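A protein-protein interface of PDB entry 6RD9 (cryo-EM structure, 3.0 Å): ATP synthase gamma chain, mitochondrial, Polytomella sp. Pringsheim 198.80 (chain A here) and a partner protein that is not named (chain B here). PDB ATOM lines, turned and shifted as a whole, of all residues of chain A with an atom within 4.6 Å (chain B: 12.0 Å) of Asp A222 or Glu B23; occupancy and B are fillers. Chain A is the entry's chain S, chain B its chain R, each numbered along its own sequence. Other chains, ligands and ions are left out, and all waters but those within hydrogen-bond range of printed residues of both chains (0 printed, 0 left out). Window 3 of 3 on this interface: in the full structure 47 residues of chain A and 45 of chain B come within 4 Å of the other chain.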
ATOM      1  N   LYS A 218      13.143  -8.309  35.068  1.00  0.00           N
ATOM      2  CA  LYS A 218      12.344  -8.726  33.921  1.00  0.00           C
ATOM      3  C   LYS A 218      11.578  -7.555  33.322  1.00  0.00           C
ATOM      4  O   LYS A 218      11.280  -7.563  32.125  1.00  0.00           O
ATOM      5  CB  LYS A 218      11.389  -9.863  34.318  1.00  0.00           C
ATOM      6  CG  LYS A 218      10.656 -10.560  33.162  1.00  0.00           C
ATOM      7  CD  LYS A 218       9.247 -10.021  32.960  1.00  0.00           C
ATOM      8  CE  LYS A 218       8.584 -10.617  31.750  1.00  0.00           C
ATOM      9  NZ  LYS A 218       7.275  -9.955  31.489  1.00  0.00           N
ATOM     10  N   GLN A 219      11.328  -6.509  34.115  1.00  0.00           N
ATOM     11  CA  GLN A 219      10.615  -5.331  33.635  1.00  0.00           C
ATOM     12  C   GLN A 219      11.416  -4.523  32.627  1.00  0.00           C
ATOM     13  O   GLN A 219      10.870  -3.595  32.025  1.00  0.00           O
ATOM     14  CB  GLN A 219      10.247  -4.425  34.806  1.00  0.00           C
ATOM     15  CG  GLN A 219       9.765  -5.162  36.031  1.00  0.00           C
ATOM     16  CD  GLN A 219       9.354  -4.220  37.140  1.00  0.00           C
ATOM     17  OE1 GLN A 219       9.346  -3.001  36.965  1.00  0.00           O
ATOM     18  NE2 GLN A 219       9.019  -4.780  38.295  1.00  0.00           N
ATOM     19  N   LEU A 220      12.695  -4.836  32.444  1.00  0.00           N
ATOM     20  CA  LEU A 220      13.502  -4.125  31.471  1.00  0.00           C
ATOM     21  C   LEU A 220      13.780  -4.979  30.243  1.00  0.00           C
ATOM     22  O   LEU A 220      14.201  -4.457  29.206  1.00  0.00           O
ATOM     23  CB  LEU A 220      14.782  -3.650  32.150  1.00  0.00           C
ATOM     24  CG  LEU A 220      15.668  -2.630  31.455  1.00  0.00           C
ATOM     25  CD1 LEU A 220      14.829  -1.481  31.029  1.00  0.00           C
ATOM     26  CD2 LEU A 220      16.589  -2.148  32.490  1.00  0.00           C
ATOM     27  N   GLU A 221      13.531  -6.277  30.318  1.00  0.00           N
ATOM     28  CA  GLU A 221      13.698  -7.128  29.151  1.00  0.00           C
ATOM     29  C   GLU A 221      12.447  -7.203  28.279  1.00  0.00           C
ATOM     30  O   GLU A 221      12.562  -7.497  27.086  1.00  0.00           O
ATOM     31  CB  GLU A 221      14.092  -8.546  29.587  1.00  0.00           C
ATOM     32  CG  GLU A 221      15.098  -8.618  30.716  1.00  0.00           C
ATOM     33  CD  GLU A 221      16.521  -8.507  30.238  1.00  0.00           C
ATOM     34  OE1 GLU A 221      16.780  -8.776  29.048  1.00  0.00           O
ATOM     35  OE2 GLU A 221      17.386  -8.136  31.049  1.00  0.00           O
ATOM     36  N   ASP A 222      11.265  -6.922  28.837  1.00  0.00           N
ATOM     37  CA  ASP A 222       9.992  -7.269  28.201  1.00  0.00           C
ATOM     38  C   ASP A 222       9.560  -6.174  27.236  1.00  0.00           C
ATOM     39  O   ASP A 222       8.657  -5.377  27.496  1.00  0.00           O
ATOM     40  CB  ASP A 222       8.927  -7.538  29.256  1.00  0.00           C
ATOM     41  CG  ASP A 222       8.878  -6.472  30.320  1.00  0.00           C
ATOM     42  OD1 ASP A 222       9.706  -5.551  30.263  1.00  0.00           O
ATOM     43  OD2 ASP A 222       8.003  -6.548  31.203  1.00  0.00           O
ATOM     44  N   VAL A 223      10.204  -6.153  26.080  1.00  0.00           N
ATOM     45  CA  VAL A 223       9.844  -5.227  25.016  1.00  0.00           C
ATOM     46  C   VAL A 223       9.403  -6.030  23.797  1.00  0.00           C
ATOM     47  O   VAL A 223      10.183  -6.819  23.243  1.00  0.00           O
ATOM     48  CB  VAL A 223      10.985  -4.245  24.710  1.00  0.00           C
ATOM     49  CG1 VAL A 223      11.013  -3.183  25.778  1.00  0.00           C
ATOM     50  CG2 VAL A 223      12.333  -4.953  24.731  1.00  0.00           C
ATOM     51  N   THR A 224       8.135  -5.836  23.407  1.00  0.00           N
ATOM     52  CA  THR A 224       7.419  -6.563  22.350  1.00  0.00           C
ATOM     53  C   THR A 224       7.521  -8.078  22.554  1.00  0.00           C
ATOM     54  O   THR A 224       7.824  -8.842  21.641  1.00  0.00           O
ATOM     55  CB  THR A 224       7.913  -6.169  20.950  1.00  0.00           C
ATOM     56  OG1 THR A 224       9.272  -6.589  20.772  1.00  0.00           O
ATOM     57  CG2 THR A 224       7.826  -4.667  20.761  1.00  0.00           C
ATOM     58  N   GLY A 225       7.207  -8.487  23.782  1.00  0.00           N
ATOM     59  CA  GLY A 225       7.464  -9.843  24.227  1.00  0.00           C
ATOM     60  C   GLY A 225       8.358  -9.869  25.448  1.00  0.00           C
ATOM     61  O   GLY A 225       7.997  -9.295  26.478  1.00  0.00           O
ATOM     62  N   ASN A 226       9.516 -10.525  25.348  1.00  0.00           N
ATOM     63  CA  ASN A 226      10.503 -10.585  26.421  1.00  0.00           C
ATOM     64  C   ASN A 226      11.816 -11.091  25.849  1.00  0.00           C
ATOM     65  O   ASN A 226      11.834 -11.884  24.905  1.00  0.00           O
ATOM     66  CB  ASN A 226      10.058 -11.495  27.566  1.00  0.00           C
ATOM     67  CG  ASN A 226      10.785 -11.207  28.850  1.00  0.00           C
ATOM     68  OD1 ASN A 226      11.340 -10.139  29.029  1.00  0.00           O
ATOM     69  ND2 ASN A 226      10.791 -12.170  29.754  1.00  0.00           N
ATOM     70  N   GLU B  23       5.729  -0.556  29.482  1.00  0.00           N
ATOM     71  CA  GLU B  23       6.596  -1.643  29.924  1.00  0.00           C
ATOM     72  C   GLU B  23       8.048  -1.365  29.556  1.00  0.00           C
ATOM     73  O   GLU B  23       8.940  -2.150  29.872  1.00  0.00           O
ATOM     74  CB  GLU B  23       6.144  -2.969  29.313  1.00  0.00           C
ATOM     75  CG  GLU B  23       6.353  -3.065  27.805  1.00  0.00           C
ATOM     76  CD  GLU B  23       5.167  -2.572  26.998  1.00  0.00           C
ATOM     77  OE1 GLU B  23       4.262  -1.932  27.571  1.00  0.00           O
ATOM     78  OE2 GLU B  23       5.149  -2.822  25.776  1.00  0.00           O
ATOM     79  N   ALA B  24       8.271  -0.235  28.892  1.00  0.00           N
ATOM     80  CA  ALA B  24       9.582   0.184  28.406  1.00  0.00           C
ATOM     81  C   ALA B  24       9.890   1.598  28.880  1.00  0.00           C
ATOM     82  O   ALA B  24      10.169   2.502  28.091  1.00  0.00           O
ATOM     83  CB  ALA B  24       9.650   0.100  26.886  1.00  0.00           C
ATOM     84  N   ALA B  25       9.832   1.802  30.199  1.00  0.00           N
ATOM     85  CA  ALA B  25       9.954   3.139  30.768  1.00  0.00           C
ATOM     86  C   ALA B  25      11.383   3.671  30.767  1.00  0.00           C
ATOM     87  O   ALA B  25      11.571   4.892  30.751  1.00  0.00           O
ATOM     88  CB  ALA B  25       9.404   3.145  32.198  1.00  0.00           C
ATOM     89  N   ALA B  26      12.392   2.801  30.790  1.00  0.00           N
ATOM     90  CA  ALA B  26      13.783   3.219  30.966  1.00  0.00           C
ATOM     91  C   ALA B  26      14.657   2.645  29.860  1.00  0.00           C
ATOM     92  O   ALA B  26      15.185   1.535  30.000  1.00  0.00           O
ATOM     93  CB  ALA B  26      14.308   2.786  32.334  1.00  0.00           C
ATOM     94  N   PRO B  27      14.866   3.366  28.764  1.00  0.00           N
ATOM     95  CA  PRO B  27      15.779   2.860  27.728  1.00  0.00           C
ATOM     96  C   PRO B  27      17.230   2.933  28.174  1.00  0.00           C
ATOM     97  O   PRO B  27      17.965   3.846  27.791  1.00  0.00           O
ATOM     98  CB  PRO B  27      15.508   3.779  26.530  1.00  0.00           C
ATOM     99  CG  PRO B  27      14.194   4.453  26.839  1.00  0.00           C
ATOM    100  CD  PRO B  27      14.151   4.573  28.327  1.00  0.00           C
ATOM    101  N   ALA B  28      17.648   1.961  28.979  1.00  0.00           N
ATOM    102  CA  ALA B  28      18.962   1.957  29.600  1.00  0.00           C
ATOM    103  C   ALA B  28      20.001   1.369  28.651  1.00  0.00           C
ATOM    104  O   ALA B  28      19.786   1.247  27.444  1.00  0.00           O
ATOM    105  CB  ALA B  28      18.921   1.182  30.910  1.00  0.00           C
ATOM    106  N   VAL B  60      22.282 -13.231  22.053  1.00  0.00           N
ATOM    107  CA  VAL B  60      21.449 -13.168  20.855  1.00  0.00           C
ATOM    108  C   VAL B  60      22.250 -12.951  19.585  1.00  0.00           C
ATOM    109  O   VAL B  60      21.672 -12.992  18.491  1.00  0.00           O
ATOM    110  CB  VAL B  60      20.398 -12.049  20.961  1.00  0.00           C
ATOM    111  CG1 VAL B  60      19.389 -12.364  22.053  1.00  0.00           C
ATOM    112  CG2 VAL B  60      21.076 -10.718  21.215  1.00  0.00           C
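The backbone carbonyl oxygen (O) of Gln A219 sits close to the backbone carbonyl oxygen (O) of Glu B23 (3.2 Å).
CD1 of Leu A220 touches O of Ala B26 (3.2 Å). Glu B23 touches Asp A222 (CG to O, 3.3 Å). Ala B24 touches Val A223 (CB to CG1, 3.7 Å).
No residue of chain B comes within 4 Å of Lys A218. Gln A219 touches just one residue of chain B: Glu B23. Printed residues of chain B within 4 Å of Leu A220: Ala B26 (3.2 Å). No residue of chain B comes within 4 Å of Glu A221. Asp A222 touches one residue of chain B. Val A223 touches just one residue of chain B: Ala B24. No residue of chain B comes within 4 Å of Thr A224. No residue of chain B comes within 4 Å of Gly A225. Of chain A, only Gln A219 and Asp A222 come within 4 Å of Glu B23. Of the printed residues of chain A, Ala B24 touches Val A223 (3.7 Å). Of the printed residues of chain A, Ala B26 touches Leu A220 (3.2 Å). The nearest residue of chain B that does not touch Asp A222 is Ala B24 (5.3 Å).
Of the 7 printed residues of chain B, 3 touch a printed residue of chain A. Printed residues of chain B that touch a printed residue of chain A: Glu B23, Ala B24 and Ala B26. Hydrophobic or aromatic side chains of chain B that line the printed part of chain A: Ala B24. Among the printed residues, no Asp or Glu carboxylate lies within 4 Å of a Lys or Arg side-chain nitrogen of the other chain.
The side-chain carboxylate (OD2) of Asp A222 lies within salt-bridge range of the side-chain amino group (NZ) of Lys A218 (3.5 Å). N of Asp A222 is in hydrogen-bond range of OD1 of Asn A226 (3.2 Å).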
